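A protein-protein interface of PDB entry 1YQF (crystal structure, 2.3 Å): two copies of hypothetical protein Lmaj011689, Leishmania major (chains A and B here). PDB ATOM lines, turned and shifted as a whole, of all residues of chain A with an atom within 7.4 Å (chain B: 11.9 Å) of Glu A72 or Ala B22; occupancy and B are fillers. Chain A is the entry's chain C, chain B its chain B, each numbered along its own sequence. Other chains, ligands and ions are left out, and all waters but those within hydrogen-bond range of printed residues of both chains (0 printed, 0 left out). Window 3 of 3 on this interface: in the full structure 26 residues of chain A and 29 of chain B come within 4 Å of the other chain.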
ATOM      1  N   SER A  70     -13.363  16.108  18.792  1.00  0.00           N
ATOM      2  CA  SER A  70     -12.356  16.982  18.205  1.00  0.00           C
ATOM      3  C   SER A  70     -12.380  16.831  16.684  1.00  0.00           C
ATOM      4  O   SER A  70     -12.813  15.805  16.160  1.00  0.00           O
ATOM      5  CB  SER A  70     -10.965  16.662  18.767  1.00  0.00           C
ATOM      6  OG  SER A  70     -10.429  17.787  19.453  1.00  0.00           O
ATOM      7  N   PHE A  71     -11.924  17.859  15.979  1.00  0.00           N
ATOM      8  CA  PHE A  71     -11.931  17.855  14.518  1.00  0.00           C
ATOM      9  C   PHE A  71     -10.889  18.823  13.982  1.00  0.00           C
ATOM     10  O   PHE A  71     -11.110  20.038  13.986  1.00  0.00           O
ATOM     11  CB  PHE A  71     -13.311  18.240  13.968  1.00  0.00           C
ATOM     12  CG  PHE A  71     -13.432  18.061  12.480  1.00  0.00           C
ATOM     13  CD1 PHE A  71     -13.757  16.821  11.947  1.00  0.00           C
ATOM     14  CD2 PHE A  71     -13.202  19.122  11.610  1.00  0.00           C
ATOM     15  CE1 PHE A  71     -13.863  16.643  10.575  1.00  0.00           C
ATOM     16  CE2 PHE A  71     -13.307  18.949  10.233  1.00  0.00           C
ATOM     17  CZ  PHE A  71     -13.639  17.706   9.717  1.00  0.00           C
ATOM     18  N   GLU A  72      -9.762  18.277  13.519  1.00  0.00           N
ATOM     19  CA  GLU A  72      -8.680  19.083  12.951  1.00  0.00           C
ATOM     20  C   GLU A  72      -8.256  20.210  13.898  1.00  0.00           C
ATOM     21  O   GLU A  72      -8.073  21.355  13.478  1.00  0.00           O
ATOM     22  CB  GLU A  72      -9.098  19.643  11.583  1.00  0.00           C
ATOM     23  CG  GLU A  72      -9.482  18.573  10.566  1.00  0.00           C
ATOM     24  CD  GLU A  72      -9.914  19.140   9.220  1.00  0.00           C
ATOM     25  OE1 GLU A  72      -9.919  20.379   9.046  1.00  0.00           O
ATOM     26  OE2 GLU A  72     -10.252  18.338   8.323  1.00  0.00           O
ATOM     27  N   GLY A  73      -8.120  19.875  15.181  1.00  0.00           N
ATOM     28  CA  GLY A  73      -7.709  20.826  16.204  1.00  0.00           C
ATOM     29  C   GLY A  73      -8.846  21.608  16.848  1.00  0.00           C
ATOM     30  O   GLY A  73      -8.641  22.283  17.859  1.00  0.00           O
ATOM     31  N   GLU A  74     -10.039  21.520  16.261  1.00  0.00           N
ATOM     32  CA  GLU A  74     -11.225  22.216  16.755  1.00  0.00           C
ATOM     33  C   GLU A  74     -11.967  21.375  17.793  1.00  0.00           C
ATOM     34  O   GLU A  74     -12.033  20.156  17.674  1.00  0.00           O
ATOM     35  CB  GLU A  74     -12.176  22.516  15.593  1.00  0.00           C
ATOM     36  CG  GLU A  74     -11.582  23.406  14.509  1.00  0.00           C
ATOM     37  CD  GLU A  74     -12.379  23.391  13.218  1.00  0.00           C
ATOM     38  OE1 GLU A  74     -13.365  22.637  13.127  1.00  0.00           O
ATOM     39  OE2 GLU A  74     -12.013  24.136  12.287  1.00  0.00           O
ATOM     40  N   ASP A  75     -12.527  22.032  18.805  1.00  0.00           N
ATOM     41  CA  ASP A  75     -13.403  21.372  19.777  1.00  0.00           C
ATOM     42  C   ASP A  75     -14.862  21.619  19.388  1.00  0.00           C
ATOM     43  O   ASP A  75     -15.305  22.761  19.348  1.00  0.00           O
ATOM     44  CB  ASP A  75     -13.151  21.925  21.184  1.00  0.00           C
ATOM     45  CG  ASP A  75     -11.789  21.535  21.737  1.00  0.00           C
ATOM     46  OD1 ASP A  75     -10.990  20.765  21.149  1.00  0.00           O
ATOM     47  OD2 ASP A  75     -11.449  22.014  22.840  1.00  0.00           O
ATOM     48  N   LEU A  76     -15.598  20.548  19.102  1.00  0.00           N
ATOM     49  CA  LEU A  76     -17.004  20.643  18.705  1.00  0.00           C
ATOM     50  C   LEU A  76     -17.925  20.243  19.849  1.00  0.00           C
ATOM     51  O   LEU A  76     -17.685  19.242  20.517  1.00  0.00           O
ATOM     52  CB  LEU A  76     -17.300  19.741  17.501  1.00  0.00           C
ATOM     53  CG  LEU A  76     -16.362  19.812  16.297  1.00  0.00           C
ATOM     54  CD1 LEU A  76     -16.906  18.944  15.171  1.00  0.00           C
ATOM     55  CD2 LEU A  76     -16.178  21.243  15.832  1.00  0.00           C
ATOM     56  N   THR A  99     -14.921  25.626  18.427  1.00  0.00           N
ATOM     57  CA  THR A  99     -13.910  26.453  19.074  1.00  0.00           C
ATOM     58  C   THR A  99     -12.521  26.185  18.495  1.00  0.00           C
ATOM     59  O   THR A  99     -12.098  25.040  18.389  1.00  0.00           O
ATOM     60  CB  THR A  99     -13.923  26.190  20.592  1.00  0.00           C
ATOM     61  OG1 THR A  99     -15.162  26.651  21.148  1.00  0.00           O
ATOM     62  CG2 THR A  99     -12.856  27.018  21.309  1.00  0.00           C
ATOM     63  N   GLN A 100     -11.828  27.258  18.126  1.00  0.00           N
ATOM     64  CA  GLN A 100     -10.456  27.189  17.630  1.00  0.00           C
ATOM     65  C   GLN A 100      -9.497  27.169  18.815  1.00  0.00           C
ATOM     66  O   GLN A 100      -9.905  27.381  19.959  1.00  0.00           O
ATOM     67  CB  GLN A 100     -10.137  28.397  16.744  1.00  0.00           C
ATOM     68  CG  GLN A 100     -11.128  28.652  15.606  1.00  0.00           C
ATOM     69  CD  GLN A 100     -10.819  27.835  14.363  1.00  0.00           C
ATOM     70  OE1 GLN A 100     -10.670  26.613  14.436  1.00  0.00           O
ATOM     71  NE2 GLN A 100     -10.722  28.507  13.221  1.00  0.00           N
ATOM     72  N   LYS A 101      -8.223  26.918  18.536  1.00  0.00           N
ATOM     73  CA  LYS A 101      -7.202  26.872  19.585  1.00  0.00           C
ATOM     74  C   LYS A 101      -7.027  28.215  20.317  1.00  0.00           C
ATOM     75  O   LYS A 101      -6.717  28.232  21.507  1.00  0.00           O
ATOM     76  CB  LYS A 101      -5.861  26.402  19.009  1.00  0.00           C
ATOM     77  CG  LYS A 101      -5.773  24.892  18.818  1.00  0.00           C
ATOM     78  CD  LYS A 101      -4.418  24.473  18.250  1.00  0.00           C
ATOM     79  CE  LYS A 101      -4.000  23.083  18.725  1.00  0.00           C
ATOM     80  NZ  LYS A 101      -4.973  22.030  18.322  1.00  0.00           N
ATOM     81  N   TYR A 165     -20.237  23.045   5.519  1.00  0.00           N
ATOM     82  CA  TYR A 165     -19.194  23.186   6.526  1.00  0.00           C
ATOM     83  C   TYR A 165     -19.572  22.454   7.816  1.00  0.00           C
ATOM     84  O   TYR A 165     -18.738  21.791   8.433  1.00  0.00           O
ATOM     85  CB  TYR A 165     -18.954  24.676   6.794  1.00  0.00           C
ATOM     86  CG  TYR A 165     -18.035  24.983   7.952  1.00  0.00           C
ATOM     87  CD1 TYR A 165     -18.532  25.096   9.246  1.00  0.00           C
ATOM     88  CD2 TYR A 165     -16.673  25.188   7.752  1.00  0.00           C
ATOM     89  CE1 TYR A 165     -17.703  25.385  10.308  1.00  0.00           C
ATOM     90  CE2 TYR A 165     -15.831  25.480   8.815  1.00  0.00           C
ATOM     91  CZ  TYR A 165     -16.355  25.578  10.094  1.00  0.00           C
ATOM     92  OH  TYR A 165     -15.536  25.866  11.164  1.00  0.00           O
ATOM     93  N   LYS A 168     -19.830  18.413   7.042  1.00  0.00           N
ATOM     94  CA  LYS A 168     -18.556  17.702   6.980  1.00  0.00           C
ATOM     95  C   LYS A 168     -18.011  17.400   8.379  1.00  0.00           C
ATOM     96  O   LYS A 168     -17.273  16.435   8.564  1.00  0.00           O
ATOM     97  CB  LYS A 168     -17.521  18.476   6.147  1.00  0.00           C
ATOM     98  CG  LYS A 168     -17.084  19.820   6.722  1.00  0.00           C
ATOM     99  CD  LYS A 168     -15.848  20.360   6.004  1.00  0.00           C
ATOM    100  CE  LYS A 168     -14.591  19.569   6.379  1.00  0.00           C
ATOM    101  NZ  LYS A 168     -13.343  20.239   5.918  1.00  0.00           N
ATOM    102  N   ARG A 169     -18.380  18.225   9.356  1.00  0.00           N
ATOM    103  CA  ARG A 169     -17.961  18.022  10.744  1.00  0.00           C
ATOM    104  C   ARG A 169     -18.879  17.075  11.534  1.00  0.00           C
ATOM    105  O   ARG A 169     -18.693  16.901  12.733  1.00  0.00           O
ATOM    106  CB  ARG A 169     -17.845  19.375  11.451  1.00  0.00           C
ATOM    107  CG  ARG A 169     -16.645  20.157  10.975  1.00  0.00           C
ATOM    108  CD  ARG A 169     -16.618  21.612  11.400  1.00  0.00           C
ATOM    109  NE  ARG A 169     -15.348  22.246  11.045  1.00  0.00           N
ATOM    110  CZ  ARG A 169     -14.933  22.511   9.805  1.00  0.00           C
ATOM    111  NH1 ARG A 169     -15.683  22.215   8.743  1.00  0.00           N
ATOM    112  NH2 ARG A 169     -13.752  23.093   9.620  1.00  0.00           N
ATOM    113  N   ALA B  22      -7.579  21.561   7.861  1.00  0.00           N
ATOM    114  CA  ALA B  22      -7.644  22.638   8.893  1.00  0.00           C
ATOM    115  C   ALA B  22      -9.007  23.327   8.877  1.00  0.00           C
ATOM    116  O   ALA B  22      -9.749  23.277   9.873  1.00  0.00           O
ATOM    117  CB  ALA B  22      -6.531  23.656   8.666  1.00  0.00           C
ATOM    118  N   SER B  23      -9.327  23.956   7.736  1.00  0.00           N
ATOM    119  CA  SER B  23     -10.587  24.680   7.563  1.00  0.00           C
ATOM    120  C   SER B  23     -11.261  24.265   6.240  1.00  0.00           C
ATOM    121  O   SER B  23     -10.955  23.191   5.710  1.00  0.00           O
ATOM    122  CB  SER B  23     -10.323  26.187   7.624  1.00  0.00           C
ATOM    123  OG  SER B  23      -9.506  26.521   8.749  1.00  0.00           O
ATOM    124  N   ASP B  24     -12.177  25.093   5.717  1.00  0.00           N
ATOM    125  CA  ASP B  24     -12.931  24.753   4.501  1.00  0.00           C
ATOM    126  C   ASP B  24     -12.947  25.865   3.434  1.00  0.00           C
ATOM    127  O   ASP B  24     -13.588  26.913   3.619  1.00  0.00           O
ATOM    128  CB  ASP B  24     -14.365  24.376   4.877  1.00  0.00           C
ATOM    129  CG  ASP B  24     -15.043  23.534   3.816  1.00  0.00           C
ATOM    130  OD1 ASP B  24     -14.410  22.927   2.914  1.00  0.00           O
ATOM    131  OD2 ASP B  24     -16.288  23.434   3.847  1.00  0.00           O
ATOM    132  N   ALA B  25     -12.261  25.602   2.313  1.00  0.00           N
ATOM    133  CA  ALA B  25     -12.058  26.594   1.239  1.00  0.00           C
ATOM    134  C   ALA B  25     -13.327  27.137   0.567  1.00  0.00           C
ATOM    135  O   ALA B  25     -13.366  28.305   0.190  1.00  0.00           O
ATOM    136  CB  ALA B  25     -11.114  26.022   0.172  1.00  0.00           C
ATOM    137  N   ALA B  26     -14.347  26.302   0.390  1.00  0.00           N
ATOM    138  CA  ALA B  26     -15.601  26.764  -0.217  1.00  0.00           C
ATOM    139  C   ALA B  26     -16.267  27.888   0.595  1.00  0.00           C
ATOM    140  O   ALA B  26     -16.829  28.820   0.021  1.00  0.00           O
ATOM    141  CB  ALA B  26     -16.566  25.607  -0.407  1.00  0.00           C
ATOM    142  N   LEU B  27     -16.195  27.796   1.922  1.00  0.00           N
ATOM    143  CA  LEU B  27     -16.755  28.823   2.804  1.00  0.00           C
ATOM    144  C   LEU B  27     -15.859  30.061   2.864  1.00  0.00           C
ATOM    145  O   LEU B  27     -16.347  31.177   3.034  1.00  0.00           O
ATOM    146  CB  LEU B  27     -16.976  28.263   4.217  1.00  0.00           C
ATOM    147  CG  LEU B  27     -17.615  29.201   5.253  1.00  0.00           C
ATOM    148  CD1 LEU B  27     -18.988  29.687   4.808  1.00  0.00           C
ATOM    149  CD2 LEU B  27     -17.723  28.517   6.601  1.00  0.00           C
ATOM    150  N   ALA B  28     -14.552  29.863   2.732  1.00  0.00           N
ATOM    151  CA  ALA B  28     -13.609  30.976   2.657  1.00  0.00           C
ATOM    152  C   ALA B  28     -13.907  31.849   1.439  1.00  0.00           C
ATOM    153  O   ALA B  28     -13.870  33.075   1.521  1.00  0.00           O
ATOM    154  CB  ALA B  28     -12.182  30.456   2.599  1.00  0.00           C
ATOM    155  N   MET B 198     -15.991  35.162   9.943  1.00  0.00           N
ATOM    156  CA  MET B 198     -16.329  33.853   9.379  1.00  0.00           C
ATOM    157  C   MET B 198     -15.321  33.426   8.312  1.00  0.00           C
ATOM    158  O   MET B 198     -15.002  32.243   8.194  1.00  0.00           O
ATOM    159  CB  MET B 198     -17.734  33.841   8.775  1.00  0.00           C
ATOM    160  CG  MET B 198     -18.102  32.478   8.185  1.00  0.00           C
ATOM    161  SD  MET B 198     -19.816  32.288   7.740  1.00  0.00           S
ATOM    162  CE  MET B 198     -20.516  32.027   9.361  1.00  0.00           C
ATOM    163  N   ASN B 199     -14.835  34.391   7.536  1.00  0.00           N
ATOM    164  CA  ASN B 199     -13.823  34.122   6.518  1.00  0.00           C
ATOM    165  C   ASN B 199     -12.536  33.646   7.181  1.00  0.00           C
ATOM    166  O   ASN B 199     -12.026  32.571   6.869  1.00  0.00           O
ATOM    167  CB  ASN B 199     -13.538  35.368   5.676  1.00  0.00           C
ATOM    168  CG  ASN B 199     -12.439  35.133   4.650  1.00  0.00           C
ATOM    169  OD1 ASN B 199     -12.687  34.596   3.570  1.00  0.00           O
ATOM    170  ND2 ASN B 199     -11.216  35.517   4.994  1.00  0.00           N
ATOM    171  N   LYS B 200     -12.021  34.452   8.107  1.00  0.00           N
ATOM    172  CA  LYS B 200     -10.868  34.064   8.915  1.00  0.00           C
ATOM    173  C   LYS B 200     -11.075  32.664   9.482  1.00  0.00           C
ATOM    174  O   LYS B 200     -10.153  31.855   9.506  1.00  0.00           O
ATOM    175  CB  LYS B 200     -10.640  35.068  10.056  1.00  0.00           C
ATOM    176  CG  LYS B 200      -9.537  34.681  11.048  1.00  0.00           C
ATOM    177  CD  LYS B 200     -10.064  33.780  12.186  1.00  0.00           C
ATOM    178  CE  LYS B 200      -9.006  33.532  13.253  1.00  0.00           C
ATOM    179  NZ  LYS B 200      -9.470  32.547  14.277  1.00  0.00           N
ATOM    180  N   PHE B 201     -12.299  32.391   9.923  1.00  0.00           N
ATOM    181  CA  PHE B 201     -12.660  31.118  10.543  1.00  0.00           C
ATOM    182  C   PHE B 201     -12.522  29.926   9.596  1.00  0.00           C
ATOM    183  O   PHE B 201     -12.122  28.843  10.018  1.00  0.00           O
ATOM    184  CB  PHE B 201     -14.101  31.184  11.064  1.00  0.00           C
ATOM    185  CG  PHE B 201     -14.321  30.427  12.336  1.00  0.00           C
ATOM    186  CD1 PHE B 201     -14.084  31.029  13.563  1.00  0.00           C
ATOM    187  CD2 PHE B 201     -14.773  29.117  12.308  1.00  0.00           C
ATOM    188  CE1 PHE B 201     -14.294  30.336  14.745  1.00  0.00           C
ATOM    189  CE2 PHE B 201     -14.984  28.416  13.488  1.00  0.00           C
ATOM    190  CZ  PHE B 201     -14.742  29.026  14.707  1.00  0.00           C
ATOM    191  N   ALA B 202     -12.861  30.130   8.325  1.00  0.00           N
ATOM    192  CA  ALA B 202     -12.869  29.057   7.326  1.00  0.00           C
ATOM    193  C   ALA B 202     -11.569  28.913   6.527  1.00  0.00           C
ATOM    194  O   ALA B 202     -11.512  28.110   5.590  1.00  0.00           O
ATOM    195  CB  ALA B 202     -14.035  29.262   6.363  1.00  0.00           C
ATOM    196  N   SER B 203     -10.529  29.667   6.884  1.00  0.00           N
ATOM    197  CA  SER B 203      -9.251  29.587   6.168  1.00  0.00           C
ATOM    198  C   SER B 203      -8.060  29.414   7.116  1.00  0.00           C
ATOM    199  O   SER B 203      -8.207  29.329   8.338  1.00  0.00           O
ATOM    200  CB  SER B 203      -9.057  30.824   5.280  1.00  0.00           C
ATOM    201  OG  SER B 203      -9.263  32.023   6.012  1.00  0.00           O
ATOM    202  OXT SER B 203      -6.901  29.339   6.680  1.00  0.00           O
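The backbone carbonyl oxygen (O) of Ala B22 sits close to the side-chain carboxylate (OE2) of Glu A74.
The backbone NH (N) of Ala B22 lies within hydrogen-bond range of the side-chain carboxylate (OE1) of Glu A72 (2.9 Å).
NH1 of Arg A169 lies within hydrogen-bond range of O of Tyr A165 (3.1 Å).
The side-chain hydroxyl of Ser A70 sits close to the backbone carbonyl oxygen of Glu A74 (3.4 Å).
OG of Ser B23 lies within hydrogen-bond range of O of Ser B203 (3.1 Å).
The side-chain carboxylate (OE1) of Glu A74 lies within salt-bridge range of the guanidinium group (NE) of Arg A169, 2.9 Å away.
N of Asp B24 sits at hydrogen-bond distance from O of Ala B202, 3.1 Å away.
Among the printed residues, merely in contact across the chains: Tyr A165 with Phe B201 (3.5 Å), Gln A100 with Phe B201 (3.5 Å), Tyr A165 with Leu B27 (3.7 Å), Tyr A165 with Asp B24 (3.8 Å), Lys A168 with Asp B24 (3.8 Å), Lys A168 with Ser B23 (3.8 Å) and Glu A72 with Ser B23 (3.9 Å).
Of chain B, only Ala B22 (2.9 Å) and Ser B23 (3.9 Å) come within 4 Å of Glu A72.
No residue of chain B comes within 4 Å of Ser A70.
Phe A71 touches none of the printed residues of chain B.
No residue of chain B comes within 4 Å of Gly A73.
Of the printed residues of chain A, Phe B201 touches Gln A100 and Tyr A165.
Of the printed residues of chain A, Leu B27 touches Tyr A165.
Leu A76 touches none of the printed residues of chain B.
The nearest printed residue of chain A that does not touch Ala B22 is Arg A169 (4.02 Å).
The nearest printed residue of chain B that does not touch Gln A100 is Lys B200 (4.4 Å).
Along chain B the printed residues that touch a printed residue of chain A span positions 22 to 201.
Hydrophobic or aromatic side chains of chain A that line the printed part of chain B: Tyr A165.
Along chain A the printed residues that touch a printed residue of chain B span positions 72 to 168.
No position is printed for both chains.
Of the 9 pairs that touch across the chains among the printed residues, none has its exchanged pair printed and touching as well.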
